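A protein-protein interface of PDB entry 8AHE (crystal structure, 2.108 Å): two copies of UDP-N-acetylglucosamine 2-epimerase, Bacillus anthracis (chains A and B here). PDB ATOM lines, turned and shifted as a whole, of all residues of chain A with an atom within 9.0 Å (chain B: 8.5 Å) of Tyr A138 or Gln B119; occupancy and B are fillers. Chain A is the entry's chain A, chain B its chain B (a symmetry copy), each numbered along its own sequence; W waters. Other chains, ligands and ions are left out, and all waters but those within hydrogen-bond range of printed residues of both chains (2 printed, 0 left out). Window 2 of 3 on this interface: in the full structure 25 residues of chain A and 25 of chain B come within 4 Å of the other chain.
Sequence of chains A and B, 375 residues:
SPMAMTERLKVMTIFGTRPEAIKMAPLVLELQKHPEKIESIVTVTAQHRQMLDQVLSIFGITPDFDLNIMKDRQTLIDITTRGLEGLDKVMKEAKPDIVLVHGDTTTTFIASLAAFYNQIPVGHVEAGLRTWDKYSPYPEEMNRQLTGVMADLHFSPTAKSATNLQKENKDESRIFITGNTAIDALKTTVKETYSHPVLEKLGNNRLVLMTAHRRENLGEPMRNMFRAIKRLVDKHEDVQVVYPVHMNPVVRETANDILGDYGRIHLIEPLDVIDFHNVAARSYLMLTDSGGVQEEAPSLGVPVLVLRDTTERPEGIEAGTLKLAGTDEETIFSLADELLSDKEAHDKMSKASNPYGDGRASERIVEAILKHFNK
The side-chain hydroxyl (OH) of Tyr A138 sits at hydrogen-bond distance from the backbone carbonyl oxygen (O) of Phe B116 (2.7 Å). OH of Tyr A138 sits close to O of Tyr B117 (3.4 Å). The side-chain amino group (NZ) of Lys A134 is in salt-bridge range of the side-chain carboxylate (OD1) of Asp B152 (2.5 Å).
The backbone NH (N) of Ile B120 lies within hydrogen-bond range of the backbone carbonyl oxygen (O) of Ala B115 (2.7 Å). ND2 of Asn B118 is in hydrogen-bond range of OD1 of Asp B88 (2.7 Å). The side-chain carboxylate of Asp A133 sits close to the backbone NH of Tyr A135 (3.2 Å). OD2 of Asp B88 lies within salt-bridge range of NZ of Lys B92 (2.9 Å). O of Val B122 lies within hydrogen-bond range of N of Asp B152 (2.7 Å).
Among the printed residues, pairs that only touch across the chains: Met A142 with Phe B116, Lys A134 with Phe B116, Tyr A135 with Gln B119, Tyr A138 with Gln B119, Ile A77 with Asp B88, Ile A77 with Tyr B117, Tyr A135 with Ile B120, Leu A76 with Tyr B117 and Tyr A135 with Phe B116.
Of the printed residues of chain B, Leu A76 touches Tyr B117 (3.9 Å). Of the printed residues of chain B, Lys A134 touches Phe B116 and Asp B152. Tyr A138 touches just these residues of chain B: Phe B116 (2.7 Å), Tyr B117 (3.3 Å) and Gln B119 (3.5 Å). Of the printed residues of chain A, Asp B88 touches Ile A77. Ile B98 touches none of the printed residues of chain A. Gln B119 touches two residues of chain A. Printed residues of chain A within 4 Å of Asp B152: Lys A134 (2.5 Å). The nearest printed residue of chain A that does not touch Asp B152 is Tyr A135 (4.7 Å).
Of the 17 printed residues of chain A, 6 touch a printed residue of chain B. Hydrophobic or aromatic side chains of chain A that line the printed part of chain B: Leu A76, Ile A77, Tyr A135, Tyr A138 and Met A142. Along chain A the printed residues that touch a printed residue of chain B span positions 76 to 142. Printed residues of chain B that touch a printed residue of chain A: Asp B88, Phe B116, Tyr B117, Gln B119, Ile B120 and Asp B152. Hydrophobic or aromatic side chains of chain B within 4 Å of the printed part of chain A: Phe B116 and Tyr B117. Among the printed residues, 12 pairs touch across the chains. Among the printed residues, Asp or Glu carboxylates within 4 Å of a Lys or Arg side-chain nitrogen of the other chain: Lys A134 with Asp B152.
No position is printed for both chains.
Water W1 lies within hydrogen-bond range of OG1 of Thr A106 (2.5 Å), OD1 of Asn A143 (2.7 Å) and OH of Tyr B117 (2.8 Å). Water W2 lies within hydrogen-bond range of the side-chain hydroxyl of Tyr A135 (2.5 Å), the backbone carbonyl oxygen of Ile B120 (2.7 Å) and the side-chain amino group of Lys A134 (2.9 Å).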
ATOM      1  N   LEU A  76     -12.492  21.038 -31.158  1.00  0.00           N
ATOM      2  CA  LEU A  76     -11.679  21.033 -29.949  1.00  0.00           C
ATOM      3  C   LEU A  76     -11.409  19.624 -29.451  1.00  0.00           C
ATOM      4  O   LEU A  76     -10.283  19.369 -29.032  1.00  0.00           O
ATOM      5  CB  LEU A  76     -12.386  21.809 -28.823  1.00  0.00           C
ATOM      6  CG  LEU A  76     -12.099  23.294 -28.791  1.00  0.00           C
ATOM      7  CD1 LEU A  76     -12.909  23.963 -27.685  1.00  0.00           C
ATOM      8  CD2 LEU A  76     -10.601  23.527 -28.665  1.00  0.00           C
ATOM      9  N   ILE A  77     -12.456  18.768 -29.367  1.00  0.00           N
ATOM     10  CA  ILE A  77     -12.307  17.398 -28.875  1.00  0.00           C
ATOM     11  C   ILE A  77     -11.309  16.682 -29.790  1.00  0.00           C
ATOM     12  O   ILE A  77     -10.377  16.045 -29.271  1.00  0.00           O
ATOM     13  CB  ILE A  77     -13.636  16.609 -28.843  1.00  0.00           C
ATOM     14  CG1 ILE A  77     -14.608  17.160 -27.814  1.00  0.00           C
ATOM     15  CG2 ILE A  77     -13.387  15.129 -28.561  1.00  0.00           C
ATOM     16  CD1 ILE A  77     -14.290  16.715 -26.405  1.00  0.00           C
ATOM     17  N   ASP A 104      -0.961  30.094 -25.436  1.00  0.00           N
ATOM     18  CA  ASP A 104      -2.304  29.745 -24.998  1.00  0.00           C
ATOM     19  C   ASP A 104      -3.026  28.912 -26.043  1.00  0.00           C
ATOM     20  O   ASP A 104      -4.274  28.846 -26.013  1.00  0.00           O
ATOM     21  CB  ASP A 104      -3.168  30.946 -24.566  1.00  0.00           C
ATOM     22  CG  ASP A 104      -2.692  32.333 -24.982  1.00  0.00           C
ATOM     23  OD1 ASP A 104      -1.835  32.958 -24.212  1.00  0.00           O
ATOM     24  OD2 ASP A 104      -3.210  32.799 -26.034  1.00  0.00           O
ATOM     25  N   THR A 106      -4.399  25.361 -27.820  1.00  0.00           N
ATOM     26  CA  THR A 106      -4.837  24.057 -27.361  1.00  0.00           C
ATOM     27  C   THR A 106      -3.660  23.074 -27.376  1.00  0.00           C
ATOM     28  O   THR A 106      -3.572  22.250 -26.478  1.00  0.00           O
ATOM     29  CB  THR A 106      -6.078  23.553 -28.112  1.00  0.00           C
ATOM     30  OG1 THR A 106      -7.139  24.398 -27.653  1.00  0.00           O
ATOM     31  CG2 THR A 106      -6.478  22.132 -27.769  1.00  0.00           C
ATOM     32  N   THR A 131      -7.235  37.317 -18.496  1.00  0.00           N
ATOM     33  CA  THR A 131      -8.491  38.072 -18.549  1.00  0.00           C
ATOM     34  C   THR A 131      -9.446  37.666 -17.423  1.00  0.00           C
ATOM     35  O   THR A 131     -10.338  38.444 -17.108  1.00  0.00           O
ATOM     36  CB  THR A 131      -9.201  37.939 -19.908  1.00  0.00           C
ATOM     37  OG1 THR A 131      -9.676  36.617 -20.119  1.00  0.00           O
ATOM     38  CG2 THR A 131      -8.298  38.303 -21.070  1.00  0.00           C
ATOM     39  N   ASP A 133     -11.737  35.657 -17.652  1.00  0.00           N
ATOM     40  CA  ASP A 133     -12.964  35.300 -18.348  1.00  0.00           C
ATOM     41  C   ASP A 133     -12.692  34.052 -19.206  1.00  0.00           C
ATOM     42  O   ASP A 133     -12.003  34.140 -20.235  1.00  0.00           O
ATOM     43  CB  ASP A 133     -13.450  36.464 -19.226  1.00  0.00           C
ATOM     44  CG  ASP A 133     -14.818  36.240 -19.845  1.00  0.00           C
ATOM     45  OD1 ASP A 133     -15.359  35.109 -19.726  1.00  0.00           O
ATOM     46  OD2 ASP A 133     -15.340  37.214 -20.385  1.00  0.00           O
ATOM     47  N   LYS A 134     -13.290  32.913 -18.803  1.00  0.00           N
ATOM     48  CA  LYS A 134     -12.931  31.610 -19.324  1.00  0.00           C
ATOM     49  C   LYS A 134     -13.533  31.435 -20.716  1.00  0.00           C
ATOM     50  O   LYS A 134     -13.117  30.527 -21.447  1.00  0.00           O
ATOM     51  CB  LYS A 134     -13.275  30.520 -18.290  1.00  0.00           C
ATOM     52  CG  LYS A 134     -14.716  30.496 -17.807  1.00  0.00           C
ATOM     53  CD  LYS A 134     -14.973  29.479 -16.703  1.00  0.00           C
ATOM     54  CE  LYS A 134     -15.207  28.086 -17.243  1.00  0.00           C
ATOM     55  NZ  LYS A 134     -15.966  27.203 -16.320  1.00  0.00           N
ATOM     56  N   TYR A 135     -14.459  32.341 -21.104  1.00  0.00           N
ATOM     57  CA  TYR A 135     -15.078  32.309 -22.435  1.00  0.00           C
ATOM     58  C   TYR A 135     -14.683  33.521 -23.273  1.00  0.00           C
ATOM     59  O   TYR A 135     -15.176  33.629 -24.411  1.00  0.00           O
ATOM     60  CB  TYR A 135     -16.615  32.182 -22.375  1.00  0.00           C
ATOM     61  CG  TYR A 135     -17.126  31.002 -21.570  1.00  0.00           C
ATOM     62  CD1 TYR A 135     -16.523  29.749 -21.624  1.00  0.00           C
ATOM     63  CD2 TYR A 135     -18.213  31.143 -20.718  1.00  0.00           C
ATOM     64  CE1 TYR A 135     -16.993  28.688 -20.860  1.00  0.00           C
ATOM     65  CE2 TYR A 135     -18.687  30.083 -19.963  1.00  0.00           C
ATOM     66  CZ  TYR A 135     -18.078  28.856 -20.023  1.00  0.00           C
ATOM     67  OH  TYR A 135     -18.552  27.841 -19.244  1.00  0.00           O
ATOM     68  N   SER A 136     -13.714  34.334 -22.794  1.00  0.00           N
ATOM     69  CA  SER A 136     -13.149  35.406 -23.611  1.00  0.00           C
ATOM     70  C   SER A 136     -11.708  35.677 -23.185  1.00  0.00           C
ATOM     71  O   SER A 136     -11.498  36.302 -22.147  1.00  0.00           O
ATOM     72  CB  SER A 136     -14.012  36.690 -23.546  1.00  0.00           C
ATOM     73  OG  SER A 136     -13.620  37.637 -24.563  1.00  0.00           O
ATOM     74  N   PRO A 137     -10.682  35.280 -23.989  1.00  0.00           N
ATOM     75  CA  PRO A 137     -10.879  34.488 -25.217  1.00  0.00           C
ATOM     76  C   PRO A 137     -11.070  32.987 -24.948  1.00  0.00           C
ATOM     77  O   PRO A 137     -10.504  32.471 -23.985  1.00  0.00           O
ATOM     78  CB  PRO A 137      -9.589  34.727 -25.998  1.00  0.00           C
ATOM     79  CG  PRO A 137      -8.552  34.848 -24.857  1.00  0.00           C
ATOM     80  CD  PRO A 137      -9.274  35.599 -23.758  1.00  0.00           C
ATOM     81  N   TYR A 138     -11.864  32.309 -25.795  1.00  0.00           N
ATOM     82  CA  TYR A 138     -12.162  30.883 -25.730  1.00  0.00           C
ATOM     83  C   TYR A 138     -11.545  30.135 -26.904  1.00  0.00           C
ATOM     84  O   TYR A 138     -11.846  30.434 -28.056  1.00  0.00           O
ATOM     85  CB  TYR A 138     -13.661  30.661 -25.798  1.00  0.00           C
ATOM     86  CG  TYR A 138     -14.108  29.226 -25.670  1.00  0.00           C
ATOM     87  CD1 TYR A 138     -14.265  28.625 -24.431  1.00  0.00           C
ATOM     88  CD2 TYR A 138     -14.393  28.472 -26.806  1.00  0.00           C
ATOM     89  CE1 TYR A 138     -14.714  27.319 -24.316  1.00  0.00           C
ATOM     90  CE2 TYR A 138     -14.868  27.180 -26.693  1.00  0.00           C
ATOM     91  CZ  TYR A 138     -15.025  26.595 -25.447  1.00  0.00           C
ATOM     92  OH  TYR A 138     -15.503  25.304 -25.352  1.00  0.00           O
ATOM     93  N   PRO A 139     -10.715  29.086 -26.692  1.00  0.00           N
ATOM     94  CA  PRO A 139     -10.369  28.544 -25.362  1.00  0.00           C
ATOM     95  C   PRO A 139      -9.048  28.998 -24.715  1.00  0.00           C
ATOM     96  O   PRO A 139      -8.543  28.329 -23.815  1.00  0.00           O
ATOM     97  CB  PRO A 139     -10.268  27.062 -25.739  1.00  0.00           C
ATOM     98  CG  PRO A 139      -9.527  27.099 -27.079  1.00  0.00           C
ATOM     99  CD  PRO A 139     -10.115  28.298 -27.793  1.00  0.00           C
ATOM    100  N   GLU A 140      -8.544  30.175 -25.119  1.00  0.00           N
ATOM    101  CA  GLU A 140      -7.160  30.600 -24.884  1.00  0.00           C
ATOM    102  C   GLU A 140      -6.934  30.916 -23.416  1.00  0.00           C
ATOM    103  O   GLU A 140      -5.888  30.592 -22.889  1.00  0.00           O
ATOM    104  CB  GLU A 140      -6.776  31.824 -25.739  1.00  0.00           C
ATOM    105  CG  GLU A 140      -6.390  31.423 -27.171  1.00  0.00           C
ATOM    106  CD  GLU A 140      -7.561  31.171 -28.110  1.00  0.00           C
ATOM    107  OE1 GLU A 140      -8.684  31.451 -27.730  1.00  0.00           O
ATOM    108  OE2 GLU A 140      -7.324  30.705 -29.210  1.00  0.00           O
ATOM    109  N   GLU A 141      -7.889  31.623 -22.789  1.00  0.00           N
ATOM    110  CA  GLU A 141      -7.766  31.955 -21.386  1.00  0.00           C
ATOM    111  C   GLU A 141      -7.566  30.692 -20.548  1.00  0.00           C
ATOM    112  O   GLU A 141      -6.627  30.643 -19.746  1.00  0.00           O
ATOM    113  CB  GLU A 141      -8.966  32.759 -20.878  1.00  0.00           C
ATOM    114  CG  GLU A 141      -8.922  33.128 -19.390  1.00  0.00           C
ATOM    115  CD  GLU A 141      -7.773  33.967 -18.876  1.00  0.00           C
ATOM    116  OE1 GLU A 141      -7.079  34.605 -19.694  1.00  0.00           O
ATOM    117  OE2 GLU A 141      -7.576  33.974 -17.649  1.00  0.00           O
ATOM    118  N   MET A 142      -8.451  29.701 -20.692  1.00  0.00           N
ATOM    119  CA  MET A 142      -8.375  28.459 -19.918  1.00  0.00           C
ATOM    120  C   MET A 142      -7.113  27.653 -20.274  1.00  0.00           C
ATOM    121  O   MET A 142      -6.459  27.122 -19.380  1.00  0.00           O
ATOM    122  CB  MET A 142      -9.617  27.598 -20.143  1.00  0.00           C
ATOM    123  CG  MET A 142      -9.787  26.478 -19.155  1.00  0.00           C
ATOM    124  SD  MET A 142      -9.891  27.128 -17.469  1.00  0.00           S
ATOM    125  CE  MET A 142     -11.365  28.071 -17.505  1.00  0.00           C
ATOM    126  N   ASN A 143      -6.721  27.599 -21.562  1.00  0.00           N
ATOM    127  CA  ASN A 143      -5.536  26.885 -21.989  1.00  0.00           C
ATOM    128  C   ASN A 143      -4.330  27.420 -21.219  1.00  0.00           C
ATOM    129  O   ASN A 143      -3.427  26.659 -20.878  1.00  0.00           O
ATOM    130  CB  ASN A 143      -5.262  27.002 -23.485  1.00  0.00           C
ATOM    131  CG  ASN A 143      -6.173  26.190 -24.387  1.00  0.00           C
ATOM    132  OD1 ASN A 143      -6.815  25.240 -23.974  1.00  0.00           O
ATOM    133  ND2 ASN A 143      -6.231  26.578 -25.649  1.00  0.00           N
ATOM    134  N   ARG A 144      -4.226  28.735 -21.019  1.00  0.00           N
ATOM    135  CA  ARG A 144      -3.013  29.267 -20.396  1.00  0.00           C
ATOM    136  C   ARG A 144      -3.079  29.070 -18.881  1.00  0.00           C
ATOM    137  O   ARG A 144      -2.026  28.849 -18.249  1.00  0.00           O
ATOM    138  CB  ARG A 144      -2.713  30.686 -20.876  1.00  0.00           C
ATOM    139  CG  ARG A 144      -3.698  31.778 -20.486  1.00  0.00           C
ATOM    140  CD  ARG A 144      -3.388  33.045 -21.274  1.00  0.00           C
ATOM    141  NE  ARG A 144      -4.535  33.945 -21.235  1.00  0.00           N
ATOM    142  CZ  ARG A 144      -4.924  34.754 -22.210  1.00  0.00           C
ATOM    143  NH1 ARG A 144      -4.272  34.753 -23.355  1.00  0.00           N
ATOM    144  NH2 ARG A 144      -5.989  35.522 -22.028  1.00  0.00           N
ATOM    145  N   ASP B  88     -18.278  14.053 -23.423  1.00  0.00           N
ATOM    146  CA  ASP B  88     -18.644  15.157 -24.289  1.00  0.00           C
ATOM    147  C   ASP B  88     -19.973  14.788 -24.947  1.00  0.00           C
ATOM    148  O   ASP B  88     -20.883  15.600 -24.945  1.00  0.00           O
ATOM    149  CB  ASP B  88     -17.578  15.437 -25.347  1.00  0.00           C
ATOM    150  CG  ASP B  88     -17.924  16.585 -26.275  1.00  0.00           C
ATOM    151  OD1 ASP B  88     -17.842  17.771 -25.811  1.00  0.00           O
ATOM    152  OD2 ASP B  88     -18.234  16.300 -27.444  1.00  0.00           O
ATOM    153  N   MET B  91     -22.923  15.213 -22.625  1.00  0.00           N
ATOM    154  CA  MET B  91     -23.248  16.619 -22.430  1.00  0.00           C
ATOM    155  C   MET B  91     -23.880  17.259 -23.668  1.00  0.00           C
ATOM    156  O   MET B  91     -24.699  18.152 -23.522  1.00  0.00           O
ATOM    157  CB  MET B  91     -21.985  17.396 -22.048  1.00  0.00           C
ATOM    158  CG  MET B  91     -21.608  17.073 -20.576  1.00  0.00           C
ATOM    159  SD  MET B  91     -20.044  17.700 -20.212  1.00  0.00           S
ATOM    160  CE  MET B  91     -19.632  16.692 -18.790  1.00  0.00           C
ATOM    161  N   LYS B  92     -23.515  16.845 -24.883  1.00  0.00           N
ATOM    162  CA  LYS B  92     -24.149  17.349 -26.098  1.00  0.00           C
ATOM    163  C   LYS B  92     -25.612  16.902 -26.157  1.00  0.00           C
ATOM    164  O   LYS B  92     -26.456  17.656 -26.615  1.00  0.00           O
ATOM    165  CB  LYS B  92     -23.364  16.919 -27.328  1.00  0.00           C
ATOM    166  CG  LYS B  92     -22.155  17.799 -27.623  1.00  0.00           C
ATOM    167  CD  LYS B  92     -21.326  17.287 -28.800  1.00  0.00           C
ATOM    168  CE  LYS B  92     -20.355  18.362 -29.267  1.00  0.00           C
ATOM    169  NZ  LYS B  92     -19.458  18.777 -28.144  1.00  0.00           N
ATOM    170  N   PRO B  96     -26.844  19.813 -19.874  1.00  0.00           N
ATOM    171  CA  PRO B  96     -26.969  20.339 -18.503  1.00  0.00           C
ATOM    172  C   PRO B  96     -26.590  21.811 -18.421  1.00  0.00           C
ATOM    173  O   PRO B  96     -25.771  22.298 -19.200  1.00  0.00           O
ATOM    174  CB  PRO B  96     -26.016  19.440 -17.722  1.00  0.00           C
ATOM    175  CG  PRO B  96     -24.993  19.028 -18.767  1.00  0.00           C
ATOM    176  CD  PRO B  96     -25.780  18.841 -20.049  1.00  0.00           C
ATOM    177  N   ASP B  97     -27.173  22.533 -17.468  1.00  0.00           N
ATOM    178  CA  ASP B  97     -26.794  23.908 -17.169  1.00  0.00           C
ATOM    179  C   ASP B  97     -25.573  23.938 -16.265  1.00  0.00           C
ATOM    180  O   ASP B  97     -24.884  24.950 -16.249  1.00  0.00           O
ATOM    181  CB  ASP B  97     -27.933  24.654 -16.469  1.00  0.00           C
ATOM    182  CG  ASP B  97     -29.097  24.876 -17.431  1.00  0.00           C
ATOM    183  OD1 ASP B  97     -28.842  25.527 -18.485  1.00  0.00           O
ATOM    184  OD2 ASP B  97     -30.179  24.272 -17.198  1.00  0.00           O
ATOM    185  N   ILE B  98     -25.328  22.846 -15.507  1.00  0.00           N
ATOM    186  CA  ILE B  98     -24.156  22.759 -14.640  1.00  0.00           C
ATOM    187  C   ILE B  98     -23.807  21.298 -14.459  1.00  0.00           C
ATOM    188  O   ILE B  98     -24.725  20.500 -14.349  1.00  0.00           O
ATOM    189  CB  ILE B  98     -24.330  23.468 -13.275  1.00  0.00           C
ATOM    190  CG1 ILE B  98     -23.043  23.394 -12.439  1.00  0.00           C
ATOM    191  CG2 ILE B  98     -25.507  22.916 -12.490  1.00  0.00           C
ATOM    192  CD1 ILE B  98     -22.893  24.406 -11.327  1.00  0.00           C
ATOM    193  N   VAL B  99     -22.498  20.993 -14.384  1.00  0.00           N
ATOM    194  CA  VAL B  99     -22.015  19.625 -14.146  1.00  0.00           C
ATOM    195  C   VAL B  99     -21.303  19.568 -12.815  1.00  0.00           C
ATOM    196  O   VAL B  99     -20.445  20.421 -12.568  1.00  0.00           O
ATOM    197  CB  VAL B  99     -21.049  19.152 -15.253  1.00  0.00           C
ATOM    198  CG1 VAL B  99     -20.420  17.804 -14.949  1.00  0.00           C
ATOM    199  CG2 VAL B  99     -21.786  19.074 -16.568  1.00  0.00           C
ATOM    200  N   SER B 112     -14.811  17.898 -16.245  1.00  0.00           N
ATOM    201  CA  SER B 112     -14.705  19.341 -16.261  1.00  0.00           C
ATOM    202  C   SER B 112     -14.255  19.817 -17.641  1.00  0.00           C
ATOM    203  O   SER B 112     -14.817  20.780 -18.175  1.00  0.00           O
ATOM    204  CB  SER B 112     -13.773  19.861 -15.147  1.00  0.00           C
ATOM    205  OG  SER B 112     -14.076  19.288 -13.875  1.00  0.00           O
ATOM    206  N   LEU B 113     -13.265  19.162 -18.248  1.00  0.00           N
ATOM    207  CA  LEU B 113     -12.785  19.624 -19.532  1.00  0.00           C
ATOM    208  C   LEU B 113     -13.900  19.487 -20.584  1.00  0.00           C
ATOM    209  O   LEU B 113     -14.029  20.323 -21.457  1.00  0.00           O
ATOM    210  CB  LEU B 113     -11.534  18.817 -19.926  1.00  0.00           C
ATOM    211  CG  LEU B 113     -10.861  19.287 -21.233  1.00  0.00           C
ATOM    212  CD1 LEU B 113     -10.338  20.709 -21.070  1.00  0.00           C
ATOM    213  CD2 LEU B 113      -9.731  18.365 -21.600  1.00  0.00           C
ATOM    214  N   ALA B 114     -14.671  18.398 -20.540  1.00  0.00           N
ATOM    215  CA  ALA B 114     -15.756  18.188 -21.491  1.00  0.00           C
ATOM    216  C   ALA B 114     -16.798  19.289 -21.310  1.00  0.00           C
ATOM    217  O   ALA B 114     -17.229  19.849 -22.326  1.00  0.00           O
ATOM    218  CB  ALA B 114     -16.361  16.801 -21.318  1.00  0.00           C
ATOM    219  N   ALA B 115     -17.160  19.630 -20.042  1.00  0.00           N
ATOM    220  CA  ALA B 115     -18.081  20.738 -19.736  1.00  0.00           C
ATOM    221  C   ALA B 115     -17.564  22.038 -20.362  1.00  0.00           C
ATOM    222  O   ALA B 115     -18.280  22.781 -21.010  1.00  0.00           O
ATOM    223  CB  ALA B 115     -18.239  20.938 -18.251  1.00  0.00           C
ATOM    224  N   PHE B 116     -16.278  22.324 -20.148  1.00  0.00           N
ATOM    225  CA  PHE B 116     -15.651  23.523 -20.664  1.00  0.00           C
ATOM    226  C   PHE B 116     -15.732  23.567 -22.191  1.00  0.00           C
ATOM    227  O   PHE B 116     -15.912  24.641 -22.792  1.00  0.00           O
ATOM    228  CB  PHE B 116     -14.192  23.568 -20.198  1.00  0.00           C
ATOM    229  CG  PHE B 116     -13.475  24.776 -20.682  1.00  0.00           C
ATOM    230  CD1 PHE B 116     -13.939  26.023 -20.339  1.00  0.00           C
ATOM    231  CD2 PHE B 116     -12.474  24.647 -21.623  1.00  0.00           C
ATOM    232  CE1 PHE B 116     -13.369  27.141 -20.906  1.00  0.00           C
ATOM    233  CE2 PHE B 116     -11.874  25.767 -22.147  1.00  0.00           C
ATOM    234  CZ  PHE B 116     -12.329  27.004 -21.784  1.00  0.00           C
ATOM    235  N   TYR B 117     -15.544  22.399 -22.807  1.00  0.00           N
ATOM    236  CA  TYR B 117     -15.545  22.234 -24.266  1.00  0.00           C
ATOM    237  C   TYR B 117     -16.959  22.372 -24.856  1.00  0.00           C
ATOM    238  O   TYR B 117     -17.120  22.352 -26.066  1.00  0.00           O
ATOM    239  CB  TYR B 117     -14.896  20.873 -24.589  1.00  0.00           C
ATOM    240  CG  TYR B 117     -13.391  20.897 -24.686  1.00  0.00           C
ATOM    241  CD1 TYR B 117     -12.664  22.010 -24.309  1.00  0.00           C
ATOM    242  CD2 TYR B 117     -12.700  19.826 -25.214  1.00  0.00           C
ATOM    243  CE1 TYR B 117     -11.294  22.073 -24.447  1.00  0.00           C
ATOM    244  CE2 TYR B 117     -11.328  19.876 -25.358  1.00  0.00           C
ATOM    245  CZ  TYR B 117     -10.622  20.991 -24.990  1.00  0.00           C
ATOM    246  OH  TYR B 117      -9.238  20.981 -25.105  1.00  0.00           O
ATOM    247  N   ASN B 118     -17.978  22.423 -23.987  1.00  0.00           N
ATOM    248  CA  ASN B 118     -19.356  22.699 -24.333  1.00  0.00           C
ATOM    249  C   ASN B 118     -19.815  23.973 -23.625  1.00  0.00           C
ATOM    250  O   ASN B 118     -21.000  24.311 -23.682  1.00  0.00           O
ATOM    251  CB  ASN B 118     -20.284  21.551 -23.921  1.00  0.00           C
ATOM    252  CG  ASN B 118     -20.042  20.338 -24.756  1.00  0.00           C
ATOM    253  OD1 ASN B 118     -20.480  20.275 -25.914  1.00  0.00           O
ATOM    254  ND2 ASN B 118     -19.297  19.404 -24.186  1.00  0.00           N
ATOM    255  N   GLN B 119     -18.882  24.690 -22.995  1.00  0.00           N
ATOM    256  CA  GLN B 119     -19.179  25.974 -22.364  1.00  0.00           C
ATOM    257  C   GLN B 119     -20.311  25.738 -21.356  1.00  0.00           C
ATOM    258  O   GLN B 119     -21.237  26.520 -21.279  1.00  0.00           O
ATOM    259  CB  GLN B 119     -19.563  27.046 -23.400  1.00  0.00           C
ATOM    260  CG  GLN B 119     -18.475  27.392 -24.413  1.00  0.00           C
ATOM    261  CD  GLN B 119     -18.670  28.800 -24.966  1.00  0.00           C
ATOM    262  OE1 GLN B 119     -19.739  29.408 -24.866  1.00  0.00           O
ATOM    263  NE2 GLN B 119     -17.634  29.351 -25.573  1.00  0.00           N
ATOM    264  N   ILE B 120     -20.217  24.649 -20.574  1.00  0.00           N
ATOM    265  CA  ILE B 120     -21.130  24.347 -19.473  1.00  0.00           C
ATOM    266  C   ILE B 120     -20.395  24.539 -18.148  1.00  0.00           C
ATOM    267  O   ILE B 120     -19.258  24.060 -18.033  1.00  0.00           O
ATOM    268  CB  ILE B 120     -21.602  22.885 -19.515  1.00  0.00           C
ATOM    269  CG1 ILE B 120     -22.335  22.538 -20.811  1.00  0.00           C
ATOM    270  CG2 ILE B 120     -22.433  22.560 -18.269  1.00  0.00           C
ATOM    271  CD1 ILE B 120     -22.614  21.090 -20.974  1.00  0.00           C
ATOM    272  N   PRO B 121     -21.004  25.297 -17.182  1.00  0.00           N
ATOM    273  CA  PRO B 121     -20.435  25.518 -15.851  1.00  0.00           C
ATOM    274  C   PRO B 121     -20.167  24.225 -15.075  1.00  0.00           C
ATOM    275  O   PRO B 121     -20.893  23.227 -15.250  1.00  0.00           O
ATOM    276  CB  PRO B 121     -21.522  26.313 -15.132  1.00  0.00           C
ATOM    277  CG  PRO B 121     -22.276  27.013 -16.214  1.00  0.00           C
ATOM    278  CD  PRO B 121     -22.199  26.116 -17.402  1.00  0.00           C
ATOM    279  N   VAL B 122     -19.144  24.267 -14.197  1.00  0.00           N
ATOM    280  CA  VAL B 122     -18.758  23.116 -13.360  1.00  0.00           C
ATOM    281  C   VAL B 122     -18.788  23.527 -11.884  1.00  0.00           C
ATOM    282  O   VAL B 122     -18.238  24.581 -11.520  1.00  0.00           O
ATOM    283  CB  VAL B 122     -17.339  22.656 -13.761  1.00  0.00           C
ATOM    284  CG1 VAL B 122     -16.737  21.648 -12.796  1.00  0.00           C
ATOM    285  CG2 VAL B 122     -17.319  22.169 -15.237  1.00  0.00           C
ATOM    286  N   ASP B 152     -16.529  26.624 -11.809  1.00  0.00           N
ATOM    287  CA  ASP B 152     -17.271  27.861 -11.624  1.00  0.00           C
ATOM    288  C   ASP B 152     -17.631  28.038 -10.141  1.00  0.00           C
ATOM    289  O   ASP B 152     -17.626  29.150  -9.646  1.00  0.00           O
ATOM    290  CB  ASP B 152     -18.517  27.892 -12.535  1.00  0.00           C
ATOM    291  CG  ASP B 152     -18.117  27.992 -14.002  1.00  0.00           C
ATOM    292  OD1 ASP B 152     -17.809  26.922 -14.646  1.00  0.00           O
ATOM    293  OD2 ASP B 152     -17.989  29.081 -14.457  1.00  0.00           O
HETATM  294  O   HOH W   1      -8.239  23.558 -25.539  1.00  0.00           O
HETATM  295  O   HOH W   2     -17.225  25.825 -18.484  1.00  0.00           O
